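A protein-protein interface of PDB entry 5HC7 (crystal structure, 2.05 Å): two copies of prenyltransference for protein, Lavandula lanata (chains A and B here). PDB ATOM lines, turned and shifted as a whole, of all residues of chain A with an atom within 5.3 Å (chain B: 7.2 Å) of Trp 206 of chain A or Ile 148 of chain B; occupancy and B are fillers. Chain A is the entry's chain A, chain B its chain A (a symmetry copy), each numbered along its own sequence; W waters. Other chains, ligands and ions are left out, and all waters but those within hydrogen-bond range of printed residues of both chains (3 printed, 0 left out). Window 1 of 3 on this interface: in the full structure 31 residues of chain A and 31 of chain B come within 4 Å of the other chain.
Ile 148 of chain A touches Trp 206 of chain B, and with the chains exchanged Trp 206 of chain A touches Ile 148 of chain B. Leu 205 of chain B touches its own counterpart, Leu 205 of chain A. Leu 205 of chain A touches Trp 206 of chain B, and with the chains exchanged Trp 206 of chain A touches Leu 205 of chain B. Of the 14 pairs that touch across the chains among the printed residues, 5 have their exchanged pair printed and touching as well.
The side-chain carboxylate (OE1) of Glu 171 of chain A is in salt-bridge range of the guanidinium group (NH1) of Arg 145 of chain B, 2.9 Å away. OE1 of Glu 175 of chain A lies within salt-bridge range of NH1 of Arg 145 of chain B (3.9 Å). The backbone carbonyl oxygen (O) of Trp 206 of chain A sits at hydrogen-bond distance from the guanidinium group (NE) of Arg 145 of chain B (2.8 Å). The backbone carbonyl oxygen (O) of Pro 209 of chain A is in hydrogen-bond range of the backbone NH (N) of Asn 202 of chain B.
N of Gly 144 of chain B sits at hydrogen-bond distance from O of Asn 202 of chain B (2.9 Å). The backbone NH (N) of Arg 145 of chain B sits at hydrogen-bond distance from the side-chain amide oxygen (OD1) of Asn 202 of chain B, at 3.0 Å. The side-chain carboxylate (OE1) of Glu 146 of chain B sits at hydrogen-bond distance from the side-chain amide nitrogen (ND2) of Asn 202 of chain B (2.8 Å).
Printed residues of chain B within 4 Å of Glu 171 of chain A: Arg 145 and Val 149. Of the printed residues of chain B, Glu 175 of chain A touches Arg 145 (3.9 Å). Printed residues of chain B within 4 Å of Leu 205 of chain A: Leu 205 (3.5 Å) and Trp 206 (3.95 Å). Trp 206 of chain A touches just these residues of chain B: Arg 145 (2.8 Å), Ile 148 (3.9 Å), Val 149 (3.8 Å) and Leu 205 (3.95 Å). Glu 146 of chain B touches none of the printed residues of chain A. Ile 148 of chain B touches just one residue of chain A: Trp 206 (3.9 Å). Lys 154 of chain B touches none of the printed residues of chain A. The nearest residue of chain A that does not touch Ile 148 of chain B is Ile 148 of chain A (4.03 Å). The nearest printed residue of chain A that does not touch Asn 202 of chain B is Leu 208 of chain A (5.6 Å).
Water W3 lies within hydrogen-bond range of the side-chain carboxylate of Glu 175 of chain A (2.7 Å) and the guanidinium group of Arg 145 of chain B (3.3 Å). Water W1 bridges OE1 of Glu 175 of chain A and NH2 of Arg 145 of chain B. Water W2 lies within hydrogen-bond range of the side-chain carboxylate (OE2) of Glu 171 of chain A and the side-chain carboxylate (OE2) of Glu 146 of chain B.
Printed residues of chain B that touch a printed residue of chain A: Arg 145, Ile 148, Val 149, Ala 152, Asn 202, Leu 205 and Trp 206. Hydrophobic or aromatic side chains of chain B that line the printed part of chain A: Ile 148, Val 149, Ala 152, Leu 205 and Trp 206. Of the 11 printed residues of chain A, 7 touch a printed residue of chain B. Hydrophobic or aromatic side chains of chain A within 4 Å of the printed part of chain B: Ile 148, Phe 174, Leu 205, Trp 206 and Pro 209.
Trp 206 of chain B touches Ile 148 of chain A. Ala 152 of chain B touches Phe 174 of chain A. Leu 205 of chain A touches Leu 205 of chain B. Trp 206 of chain B touches Leu 205 of chain A. CG2 of Ile 148 of chain B touches CZ3 of Trp 206 of chain A, 3.9 Å away. Trp 206 of chain A touches Leu 205 of chain B. Arg 145 of chain B touches Pro 209 of chain A (NH2 to CD, 3.4 Å). Pro 209 of chain A touches Leu 205 of chain B (CA to CD2, 3.8 Å).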
ATOM      1  N   ILE A 148      19.543 -33.783 -24.645  1.00  0.00           N
ATOM      2  CA  ILE A 148      19.218 -32.454 -24.275  1.00  0.00           C
ATOM      3  C   ILE A 148      18.699 -31.661 -25.487  1.00  0.00           C
ATOM      4  O   ILE A 148      17.728 -30.884 -25.402  1.00  0.00           O
ATOM      5  CB  ILE A 148      20.443 -31.805 -23.667  1.00  0.00           C
ATOM      6  CG1 ILE A 148      20.735 -32.395 -22.283  1.00  0.00           C
ATOM      7  CG2 ILE A 148      20.264 -30.312 -23.471  1.00  0.00           C
ATOM      8  CD1 ILE A 148      22.098 -32.058 -21.749  1.00  0.00           C
ATOM      9  N   GLU A 171      13.404 -26.870 -14.574  1.00  0.00           N
ATOM     10  CA  GLU A 171      14.026 -28.205 -14.587  1.00  0.00           C
ATOM     11  C   GLU A 171      13.053 -29.264 -14.827  1.00  0.00           C
ATOM     12  O   GLU A 171      13.283 -30.190 -15.618  1.00  0.00           O
ATOM     13  CB  GLU A 171      14.706 -28.581 -13.261  1.00  0.00           C
ATOM     14  CG  GLU A 171      15.929 -27.826 -13.025  1.00  0.00           C
ATOM     15  CD  GLU A 171      16.705 -28.324 -11.833  1.00  0.00           C
ATOM     16  OE1 GLU A 171      17.024 -29.510 -11.759  1.00  0.00           O
ATOM     17  OE2 GLU A 171      17.006 -27.487 -10.970  1.00  0.00           O
ATOM     18  N   PHE A 174      11.887 -29.444 -18.223  1.00  0.00           N
ATOM     19  CA  PHE A 174      12.972 -29.990 -19.037  1.00  0.00           C
ATOM     20  C   PHE A 174      13.116 -31.480 -18.897  1.00  0.00           C
ATOM     21  O   PHE A 174      13.195 -32.212 -19.855  1.00  0.00           O
ATOM     22  CB  PHE A 174      14.318 -29.235 -18.755  1.00  0.00           C
ATOM     23  CG  PHE A 174      15.198 -29.187 -19.954  1.00  0.00           C
ATOM     24  CD1 PHE A 174      16.047 -30.212 -20.198  1.00  0.00           C
ATOM     25  CD2 PHE A 174      15.064 -28.175 -20.885  1.00  0.00           C
ATOM     26  CE1 PHE A 174      16.850 -30.214 -21.323  1.00  0.00           C
ATOM     27  CE2 PHE A 174      15.826 -28.167 -22.023  1.00  0.00           C
ATOM     28  CZ  PHE A 174      16.707 -29.208 -22.257  1.00  0.00           C
ATOM     29  N   GLU A 175      13.057 -31.942 -17.673  1.00  0.00           N
ATOM     30  CA  GLU A 175      13.165 -33.344 -17.363  1.00  0.00           C
ATOM     31  C   GLU A 175      12.111 -34.227 -18.004  1.00  0.00           C
ATOM     32  O   GLU A 175      12.362 -35.348 -18.411  1.00  0.00           O
ATOM     33  CB  GLU A 175      13.100 -33.389 -15.811  1.00  0.00           C
ATOM     34  CG  GLU A 175      13.296 -34.698 -15.109  1.00  0.00           C
ATOM     35  CD  GLU A 175      14.749 -34.974 -14.882  1.00  0.00           C
ATOM     36  OE1 GLU A 175      15.423 -34.339 -14.032  1.00  0.00           O
ATOM     37  OE2 GLU A 175      15.216 -35.867 -15.606  1.00  0.00           O
ATOM     38  N   LEU A 178      13.082 -35.255 -21.786  1.00  0.00           N
ATOM     39  CA  LEU A 178      14.215 -36.101 -22.003  1.00  0.00           C
ATOM     40  C   LEU A 178      13.845 -37.536 -22.193  1.00  0.00           C
ATOM     41  O   LEU A 178      12.763 -37.976 -21.794  1.00  0.00           O
ATOM     42  CB  LEU A 178      15.154 -35.981 -20.806  1.00  0.00           C
ATOM     43  CG  LEU A 178      15.860 -34.678 -20.633  1.00  0.00           C
ATOM     44  CD1 LEU A 178      16.532 -34.711 -19.258  1.00  0.00           C
ATOM     45  CD2 LEU A 178      16.915 -34.440 -21.719  1.00  0.00           C
ATOM     46  N   PHE A 204      24.754 -39.856 -20.368  1.00  0.00           N
ATOM     47  CA  PHE A 204      24.000 -38.850 -19.647  1.00  0.00           C
ATOM     48  C   PHE A 204      24.835 -37.661 -19.278  1.00  0.00           C
ATOM     49  O   PHE A 204      25.961 -37.790 -18.770  1.00  0.00           O
ATOM     50  CB  PHE A 204      23.537 -39.404 -18.305  1.00  0.00           C
ATOM     51  CG  PHE A 204      22.549 -40.537 -18.395  1.00  0.00           C
ATOM     52  CD1 PHE A 204      21.535 -40.539 -19.361  1.00  0.00           C
ATOM     53  CD2 PHE A 204      22.600 -41.576 -17.507  1.00  0.00           C
ATOM     54  CE1 PHE A 204      20.605 -41.580 -19.445  1.00  0.00           C
ATOM     55  CE2 PHE A 204      21.626 -42.657 -17.543  1.00  0.00           C
ATOM     56  CZ  PHE A 204      20.605 -42.638 -18.509  1.00  0.00           C
ATOM     57  N   LEU A 205      24.221 -36.481 -19.382  1.00  0.00           N
ATOM     58  CA  LEU A 205      24.806 -35.282 -18.903  1.00  0.00           C
ATOM     59  C   LEU A 205      23.838 -34.607 -17.937  1.00  0.00           C
ATOM     60  O   LEU A 205      24.154 -34.397 -16.734  1.00  0.00           O
ATOM     61  CB  LEU A 205      25.161 -34.377 -20.118  1.00  0.00           C
ATOM     62  CG  LEU A 205      26.167 -34.890 -21.166  1.00  0.00           C
ATOM     63  CD1 LEU A 205      26.267 -33.966 -22.372  1.00  0.00           C
ATOM     64  CD2 LEU A 205      27.555 -35.074 -20.550  1.00  0.00           C
ATOM     65  N   TRP A 206      22.658 -34.221 -18.439  1.00  0.00           N
ATOM     66  CA  TRP A 206      21.622 -33.606 -17.593  1.00  0.00           C
ATOM     67  C   TRP A 206      21.385 -34.463 -16.337  1.00  0.00           C
ATOM     68  O   TRP A 206      21.188 -33.943 -15.250  1.00  0.00           O
ATOM     69  CB  TRP A 206      20.306 -33.485 -18.369  1.00  0.00           C
ATOM     70  CG  TRP A 206      19.153 -33.141 -17.481  1.00  0.00           C
ATOM     71  CD1 TRP A 206      18.403 -34.009 -16.729  1.00  0.00           C
ATOM     72  CD2 TRP A 206      18.618 -31.827 -17.244  1.00  0.00           C
ATOM     73  NE1 TRP A 206      17.436 -33.290 -16.027  1.00  0.00           N
ATOM     74  CE2 TRP A 206      17.578 -31.961 -16.295  1.00  0.00           C
ATOM     75  CE3 TRP A 206      18.952 -30.536 -17.705  1.00  0.00           C
ATOM     76  CZ2 TRP A 206      16.816 -30.883 -15.880  1.00  0.00           C
ATOM     77  CZ3 TRP A 206      18.230 -29.427 -17.200  1.00  0.00           C
ATOM     78  CH2 TRP A 206      17.176 -29.623 -16.322  1.00  0.00           C
ATOM     79  N   GLN A 207      21.433 -35.759 -16.503  1.00  0.00           N
ATOM     80  CA  GLN A 207      20.998 -36.693 -15.490  1.00  0.00           C
ATOM     81  C   GLN A 207      22.029 -36.893 -14.387  1.00  0.00           C
ATOM     82  O   GLN A 207      21.734 -37.581 -13.436  1.00  0.00           O
ATOM     83  CB  GLN A 207      20.674 -38.051 -16.109  1.00  0.00           C
ATOM     84  CG  GLN A 207      19.442 -38.060 -17.014  1.00  0.00           C
ATOM     85  CD  GLN A 207      19.683 -37.621 -18.452  1.00  0.00           C
ATOM     86  OE1 GLN A 207      20.786 -37.177 -18.856  1.00  0.00           O
ATOM     87  NE2 GLN A 207      18.633 -37.769 -19.265  1.00  0.00           N
ATOM     88  N   LEU A 208      23.182 -36.233 -14.463  1.00  0.00           N
ATOM     89  CA  LEU A 208      24.298 -36.540 -13.535  1.00  0.00           C
ATOM     90  C   LEU A 208      24.790 -35.551 -12.481  1.00  0.00           C
ATOM     91  O   LEU A 208      25.971 -35.660 -12.050  1.00  0.00           O
ATOM     92  CB  LEU A 208      25.520 -36.918 -14.388  1.00  0.00           C
ATOM     93  CG  LEU A 208      25.326 -38.146 -15.289  1.00  0.00           C
ATOM     94  CD1 LEU A 208      26.690 -38.428 -15.929  1.00  0.00           C
ATOM     95  CD2 LEU A 208      24.796 -39.442 -14.677  1.00  0.00           C
ATOM     96  N   PRO A 209      23.945 -34.584 -12.025  1.00  0.00           N
ATOM     97  CA  PRO A 209      24.535 -33.510 -11.266  1.00  0.00           C
ATOM     98  C   PRO A 209      25.032 -33.959  -9.884  1.00  0.00           C
ATOM     99  O   PRO A 209      26.004 -33.439  -9.429  1.00  0.00           O
ATOM    100  CB  PRO A 209      23.386 -32.466 -11.151  1.00  0.00           C
ATOM    101  CG  PRO A 209      22.124 -33.291 -11.322  1.00  0.00           C
ATOM    102  CD  PRO A 209      22.522 -34.324 -12.324  1.00  0.00           C
ATOM    103  N   TYR B 142      26.899 -20.402 -10.064  1.00  0.00           N
ATOM    104  CA  TYR B 142      26.799 -21.159 -11.326  1.00  0.00           C
ATOM    105  C   TYR B 142      26.417 -22.617 -11.033  1.00  0.00           C
ATOM    106  O   TYR B 142      27.003 -23.267 -10.161  1.00  0.00           O
ATOM    107  CB  TYR B 142      28.134 -21.121 -12.148  1.00  0.00           C
ATOM    108  CG  TYR B 142      27.989 -22.022 -13.346  1.00  0.00           C
ATOM    109  CD1 TYR B 142      27.413 -21.529 -14.529  1.00  0.00           C
ATOM    110  CD2 TYR B 142      28.327 -23.377 -13.271  1.00  0.00           C
ATOM    111  CE1 TYR B 142      27.191 -22.359 -15.591  1.00  0.00           C
ATOM    112  CE2 TYR B 142      28.112 -24.229 -14.331  1.00  0.00           C
ATOM    113  CZ  TYR B 142      27.554 -23.712 -15.506  1.00  0.00           C
ATOM    114  OH  TYR B 142      27.253 -24.556 -16.548  1.00  0.00           O
ATOM    115  N   GLY B 143      25.439 -23.097 -11.758  1.00  0.00           N
ATOM    116  CA  GLY B 143      25.008 -24.477 -11.681  1.00  0.00           C
ATOM    117  C   GLY B 143      24.715 -24.991 -13.091  1.00  0.00           C
ATOM    118  O   GLY B 143      24.142 -24.284 -13.915  1.00  0.00           O
ATOM    119  N   GLY B 144      25.074 -26.240 -13.366  1.00  0.00           N
ATOM    120  CA  GLY B 144      24.940 -26.769 -14.718  1.00  0.00           C
ATOM    121  C   GLY B 144      23.541 -26.953 -15.207  1.00  0.00           C
ATOM    122  O   GLY B 144      23.271 -26.683 -16.376  1.00  0.00           O
ATOM    123  N   ARG B 145      22.635 -27.426 -14.320  1.00  0.00           N
ATOM    124  CA  ARG B 145      21.213 -27.529 -14.682  1.00  0.00           C
ATOM    125  C   ARG B 145      20.629 -26.156 -14.955  1.00  0.00           C
ATOM    126  O   ARG B 145      19.903 -25.967 -15.918  1.00  0.00           O
ATOM    127  CB  ARG B 145      20.438 -28.130 -13.498  1.00  0.00           C
ATOM    128  CG  ARG B 145      20.673 -29.605 -13.263  1.00  0.00           C
ATOM    129  CD  ARG B 145      19.761 -30.393 -14.079  1.00  0.00           C
ATOM    130  NE  ARG B 145      19.887 -31.864 -13.935  1.00  0.00           N
ATOM    131  CZ  ARG B 145      19.085 -32.625 -13.198  1.00  0.00           C
ATOM    132  NH1 ARG B 145      18.150 -32.046 -12.453  1.00  0.00           N
ATOM    133  NH2 ARG B 145      19.208 -33.950 -13.168  1.00  0.00           N
ATOM    134  N   GLU B 146      20.953 -25.198 -14.104  1.00  0.00           N
ATOM    135  CA  GLU B 146      20.441 -23.843 -14.278  1.00  0.00           C
ATOM    136  C   GLU B 146      20.910 -23.273 -15.596  1.00  0.00           C
ATOM    137  O   GLU B 146      20.141 -22.575 -16.291  1.00  0.00           O
ATOM    138  CB  GLU B 146      20.964 -22.937 -13.221  1.00  0.00           C
ATOM    139  CG  GLU B 146      20.338 -23.206 -11.880  1.00  0.00           C
ATOM    140  CD  GLU B 146      20.815 -24.469 -11.158  1.00  0.00           C
ATOM    141  OE1 GLU B 146      21.753 -25.231 -11.535  1.00  0.00           O
ATOM    142  OE2 GLU B 146      20.269 -24.661 -10.097  1.00  0.00           O
ATOM    143  N   ASP B 147      22.155 -23.571 -15.970  1.00  0.00           N
ATOM    144  CA  ASP B 147      22.722 -23.110 -17.277  1.00  0.00           C
ATOM    145  C   ASP B 147      21.924 -23.673 -18.440  1.00  0.00           C
ATOM    146  O   ASP B 147      21.561 -22.985 -19.380  1.00  0.00           O
ATOM    147  CB  ASP B 147      24.164 -23.527 -17.360  1.00  0.00           C
ATOM    148  CG  ASP B 147      24.975 -22.772 -18.413  1.00  0.00           C
ATOM    149  OD1 ASP B 147      24.442 -21.819 -19.056  1.00  0.00           O
ATOM    150  OD2 ASP B 147      26.159 -23.210 -18.598  1.00  0.00           O
ATOM    151  N   ILE B 148      21.637 -24.956 -18.403  1.00  0.00           N
ATOM    152  CA  ILE B 148      20.902 -25.547 -19.462  1.00  0.00           C
ATOM    153  C   ILE B 148      19.473 -24.981 -19.517  1.00  0.00           C
ATOM    154  O   ILE B 148      18.916 -24.694 -20.594  1.00  0.00           O
ATOM    155  CB  ILE B 148      20.902 -27.049 -19.274  1.00  0.00           C
ATOM    156  CG1 ILE B 148      22.289 -27.630 -19.566  1.00  0.00           C
ATOM    157  CG2 ILE B 148      19.936 -27.744 -20.214  1.00  0.00           C
ATOM    158  CD1 ILE B 148      22.473 -29.044 -19.095  1.00  0.00           C
ATOM    159  N   VAL B 149      18.852 -24.878 -18.351  1.00  0.00           N
ATOM    160  CA  VAL B 149      17.483 -24.385 -18.289  1.00  0.00           C
ATOM    161  C   VAL B 149      17.431 -22.964 -18.898  1.00  0.00           C
ATOM    162  O   VAL B 149      16.580 -22.673 -19.728  1.00  0.00           O
ATOM    163  CB  VAL B 149      16.891 -24.451 -16.861  1.00  0.00           C
ATOM    164  CG1 VAL B 149      15.535 -23.727 -16.813  1.00  0.00           C
ATOM    165  CG2 VAL B 149      16.715 -25.881 -16.447  1.00  0.00           C
ATOM    166  N   GLU B 150      18.306 -22.107 -18.429  1.00  0.00           N
ATOM    167  CA  GLU B 150      18.420 -20.727 -18.933  1.00  0.00           C
ATOM    168  C   GLU B 150      18.722 -20.694 -20.425  1.00  0.00           C
ATOM    169  O   GLU B 150      18.084 -19.978 -21.141  1.00  0.00           O
ATOM    170  CB  GLU B 150      19.434 -19.942 -18.113  1.00  0.00           C
ATOM    171  CG  GLU B 150      19.662 -18.504 -18.571  1.00  0.00           C
ATOM    172  CD  GLU B 150      18.349 -17.681 -18.610  1.00  0.00           C
ATOM    173  OE1 GLU B 150      17.394 -18.053 -17.902  1.00  0.00           O
ATOM    174  OE2 GLU B 150      18.244 -16.702 -19.391  1.00  0.00           O
ATOM    175  N   ALA B 151      19.614 -21.534 -20.931  1.00  0.00           N
ATOM    176  CA  ALA B 151      19.720 -21.683 -22.390  1.00  0.00           C
ATOM    177  C   ALA B 151      18.418 -22.035 -23.102  1.00  0.00           C
ATOM    178  O   ALA B 151      18.091 -21.470 -24.184  1.00  0.00           O
ATOM    179  CB  ALA B 151      20.772 -22.724 -22.765  1.00  0.00           C
ATOM    180  N   ALA B 152      17.733 -23.038 -22.572  1.00  0.00           N
ATOM    181  CA  ALA B 152      16.500 -23.495 -23.167  1.00  0.00           C
ATOM    182  C   ALA B 152      15.470 -22.361 -23.172  1.00  0.00           C
ATOM    183  O   ALA B 152      14.737 -22.183 -24.142  1.00  0.00           O
ATOM    184  CB  ALA B 152      15.952 -24.729 -22.468  1.00  0.00           C
ATOM    185  N   ARG B 153      15.449 -21.587 -22.109  1.00  0.00           N
ATOM    186  CA  ARG B 153      14.522 -20.478 -22.006  1.00  0.00           C
ATOM    187  C   ARG B 153      14.820 -19.405 -23.041  1.00  0.00           C
ATOM    188  O   ARG B 153      13.912 -18.952 -23.730  1.00  0.00           O
ATOM    189  CB  ARG B 153      14.649 -19.827 -20.654  1.00  0.00           C
ATOM    190  CG  ARG B 153      13.883 -20.478 -19.553  1.00  0.00           C
ATOM    191  CD  ARG B 153      14.021 -19.625 -18.308  1.00  0.00           C
ATOM    192  NE  ARG B 153      13.662 -20.403 -17.141  1.00  0.00           N
ATOM    193  CZ  ARG B 153      12.563 -20.231 -16.425  1.00  0.00           C
ATOM    194  NH1 ARG B 153      11.687 -19.279 -16.756  1.00  0.00           N
ATOM    195  NH2 ARG B 153      12.351 -21.014 -15.363  1.00  0.00           N
ATOM    196  N   LYS B 154      16.085 -18.987 -23.162  1.00  0.00           N
ATOM    197  CA  LYS B 154      16.413 -17.990 -24.192  1.00  0.00           C
ATOM    198  C   LYS B 154      16.017 -18.448 -25.581  1.00  0.00           C
ATOM    199  O   LYS B 154      15.601 -17.652 -26.419  1.00  0.00           O
ATOM    200  CB  LYS B 154      17.896 -17.663 -24.239  1.00  0.00           C
ATOM    201  CG  LYS B 154      18.463 -16.865 -23.105  1.00  0.00           C
ATOM    202  CD  LYS B 154      19.936 -17.319 -23.028  1.00  0.00           C
ATOM    203  CE  LYS B 154      20.936 -16.222 -22.750  1.00  0.00           C
ATOM    204  NZ  LYS B 154      20.626 -15.655 -21.428  1.00  0.00           N
ATOM    205  N   ILE B 155      16.290 -19.704 -25.874  1.00  0.00           N
ATOM    206  CA  ILE B 155      16.017 -20.258 -27.194  1.00  0.00           C
ATOM    207  C   ILE B 155      14.518 -20.296 -27.425  1.00  0.00           C
ATOM    208  O   ILE B 155      14.046 -20.084 -28.555  1.00  0.00           O
ATOM    209  CB  ILE B 155      16.608 -21.648 -27.332  1.00  0.00           C
ATOM    210  CG1 ILE B 155      18.117 -21.541 -27.609  1.00  0.00           C
ATOM    211  CG2 ILE B 155      15.968 -22.417 -28.419  1.00  0.00           C
ATOM    212  CD1 ILE B 155      18.885 -22.807 -27.224  1.00  0.00           C
ATOM    213  N   PHE B 174      22.474 -24.543 -29.257  1.00  0.00           N
ATOM    214  CA  PHE B 174      22.370 -24.682 -27.805  1.00  0.00           C
ATOM    215  C   PHE B 174      23.561 -24.121 -27.077  1.00  0.00           C
ATOM    216  O   PHE B 174      23.447 -23.365 -26.143  1.00  0.00           O
ATOM    217  CB  PHE B 174      22.076 -26.169 -27.404  1.00  0.00           C
ATOM    218  CG  PHE B 174      21.266 -26.266 -26.159  1.00  0.00           C
ATOM    219  CD1 PHE B 174      21.889 -26.267 -24.958  1.00  0.00           C
ATOM    220  CD2 PHE B 174      19.887 -26.224 -26.212  1.00  0.00           C
ATOM    221  CE1 PHE B 174      21.164 -26.318 -23.783  1.00  0.00           C
ATOM    222  CE2 PHE B 174      19.143 -26.244 -25.063  1.00  0.00           C
ATOM    223  CZ  PHE B 174      19.786 -26.265 -23.838  1.00  0.00           C
ATOM    224  N   HIS B 177      23.839 -20.307 -26.326  1.00  0.00           N
ATOM    225  CA  HIS B 177      22.956 -19.688 -25.279  1.00  0.00           C
ATOM    226  C   HIS B 177      23.310 -20.071 -23.831  1.00  0.00           C
ATOM    227  O   HIS B 177      22.699 -19.594 -22.859  1.00  0.00           O
ATOM    228  CB  HIS B 177      21.500 -20.004 -25.612  1.00  0.00           C
ATOM    229  CG  HIS B 177      21.086 -19.405 -26.921  1.00  0.00           C
ATOM    230  ND1 HIS B 177      21.240 -20.069 -28.120  1.00  0.00           N
ATOM    231  CD2 HIS B 177      20.658 -18.159 -27.230  1.00  0.00           C
ATOM    232  CE1 HIS B 177      20.846 -19.284 -29.110  1.00  0.00           C
ATOM    233  NE2 HIS B 177      20.492 -18.122 -28.594  1.00  0.00           N
ATOM    234  N   LEU B 178      24.348 -20.871 -23.699  1.00  0.00           N
ATOM    235  CA  LEU B 178      24.873 -21.180 -22.405  1.00  0.00           C
ATOM    236  C   LEU B 178      25.774 -20.115 -21.870  1.00  0.00           C
ATOM    237  O   LEU B 178      26.315 -19.298 -22.620  1.00  0.00           O
ATOM    238  CB  LEU B 178      25.646 -22.493 -22.489  1.00  0.00           C
ATOM    239  CG  LEU B 178      24.846 -23.731 -22.723  1.00  0.00           C
ATOM    240  CD1 LEU B 178      25.840 -24.858 -23.016  1.00  0.00           C
ATOM    241  CD2 LEU B 178      23.984 -24.103 -21.512  1.00  0.00           C
ATOM    242  N   MET B 179      26.003 -20.151 -20.558  1.00  0.00           N
ATOM    243  CA  MET B 179      26.833 -19.145 -19.908  1.00  0.00           C
ATOM    244  C   MET B 179      28.290 -19.219 -20.316  1.00  0.00           C
ATOM    245  O   MET B 179      29.057 -18.265 -20.141  1.00  0.00           O
ATOM    246  CB  MET B 179      26.684 -19.228 -18.416  1.00  0.00           C
ATOM    247  CG  MET B 179      25.293 -18.817 -17.949  1.00  0.00           C
ATOM    248  SD  MET B 179      25.153 -18.893 -16.159  1.00  0.00           S
ATOM    249  CE  MET B 179      24.178 -20.322 -15.801  1.00  0.00           C
ATOM    250  N   ASN B 202      26.511 -30.649  -9.517  1.00  0.00           N
ATOM    251  CA  ASN B 202      25.793 -29.653 -10.288  1.00  0.00           C
ATOM    252  C   ASN B 202      26.697 -28.526 -10.776  1.00  0.00           C
ATOM    253  O   ASN B 202      26.280 -27.341 -10.939  1.00  0.00           O
ATOM    254  CB  ASN B 202      24.527 -29.115  -9.586  1.00  0.00           C
ATOM    255  CG  ASN B 202      23.637 -28.275 -10.537  1.00  0.00           C
ATOM    256  OD1 ASN B 202      23.516 -28.583 -11.705  1.00  0.00           O
ATOM    257  ND2 ASN B 202      23.044 -27.194 -10.019  1.00  0.00           N
ATOM    258  N   PHE B 204      29.238 -27.810 -14.353  1.00  0.00           N
ATOM    259  CA  PHE B 204      28.957 -28.096 -15.746  1.00  0.00           C
ATOM    260  C   PHE B 204      28.381 -29.465 -15.946  1.00  0.00           C
ATOM    261  O   PHE B 204      28.875 -30.466 -15.401  1.00  0.00           O
ATOM    262  CB  PHE B 204      30.254 -28.122 -16.546  1.00  0.00           C
ATOM    263  CG  PHE B 204      30.973 -26.802 -16.631  1.00  0.00           C
ATOM    264  CD1 PHE B 204      30.268 -25.602 -16.782  1.00  0.00           C
ATOM    265  CD2 PHE B 204      32.340 -26.751 -16.598  1.00  0.00           C
ATOM    266  CE1 PHE B 204      30.926 -24.372 -16.876  1.00  0.00           C
ATOM    267  CE2 PHE B 204      33.058 -25.491 -16.728  1.00  0.00           C
ATOM    268  CZ  PHE B 204      32.336 -24.296 -16.894  1.00  0.00           C
ATOM    269  N   LEU B 205      27.419 -29.546 -16.868  1.00  0.00           N
ATOM    270  CA  LEU B 205      26.897 -30.790 -17.305  1.00  0.00           C
ATOM    271  C   LEU B 205      27.016 -30.873 -18.823  1.00  0.00           C
ATOM    272  O   LEU B 205      27.698 -31.777 -19.378  1.00  0.00           O
ATOM    273  CB  LEU B 205      25.426 -30.917 -16.816  1.00  0.00           C
ATOM    274  CG  LEU B 205      25.136 -30.902 -15.303  1.00  0.00           C
ATOM    275  CD1 LEU B 205      23.643 -30.856 -15.002  1.00  0.00           C
ATOM    276  CD2 LEU B 205      25.756 -32.118 -14.613  1.00  0.00           C
ATOM    277  N   TRP B 206      26.335 -29.962 -19.531  1.00  0.00           N
ATOM    278  CA  TRP B 206      26.412 -29.909 -21.000  1.00  0.00           C
ATOM    279  C   TRP B 206      27.883 -29.912 -21.454  1.00  0.00           C
ATOM    280  O   TRP B 206      28.235 -30.539 -22.441  1.00  0.00           O
ATOM    281  CB  TRP B 206      25.732 -28.639 -21.521  1.00  0.00           C
ATOM    282  CG  TRP B 206      26.030 -28.387 -22.965  1.00  0.00           C
ATOM    283  CD1 TRP B 206      27.140 -27.770 -23.483  1.00  0.00           C
ATOM    284  CD2 TRP B 206      25.206 -28.754 -24.085  1.00  0.00           C
ATOM    285  NE1 TRP B 206      27.047 -27.751 -24.875  1.00  0.00           N
ATOM    286  CE2 TRP B 206      25.900 -28.379 -25.259  1.00  0.00           C
ATOM    287  CE3 TRP B 206      23.965 -29.413 -24.214  1.00  0.00           C
ATOM    288  CZ2 TRP B 206      25.359 -28.549 -26.522  1.00  0.00           C
ATOM    289  CZ3 TRP B 206      23.464 -29.670 -25.514  1.00  0.00           C
ATOM    290  CH2 TRP B 206      24.155 -29.221 -26.629  1.00  0.00           C
ATOM    291  N   GLN B 207      28.718 -29.232 -20.714  1.00  0.00           N
ATOM    292  CA  GLN B 207      30.070 -28.936 -21.131  1.00  0.00           C
ATOM    293  C   GLN B 207      31.017 -30.114 -20.948  1.00  0.00           C
ATOM    294  O   GLN B 207      32.153 -30.013 -21.353  1.00  0.00           O
ATOM    295  CB  GLN B 207      30.624 -27.739 -20.362  1.00  0.00           C
ATOM    296  CG  GLN B 207      29.955 -26.405 -20.693  1.00  0.00           C
ATOM    297  CD  GLN B 207      28.666 -26.113 -19.936  1.00  0.00           C
ATOM    298  OE1 GLN B 207      28.120 -26.945 -19.170  1.00  0.00           O
ATOM    299  NE2 GLN B 207      28.170 -24.888 -20.129  1.00  0.00           N
HETATM  300  O   HOH W   1      16.633 -35.035 -11.720  1.00  0.00           O
HETATM  301  O   HOH W   2      19.557 -27.564  -9.686  1.00  0.00           O
HETATM  302  O   HOH W   3      17.632 -36.523 -14.608  1.00  0.00           O
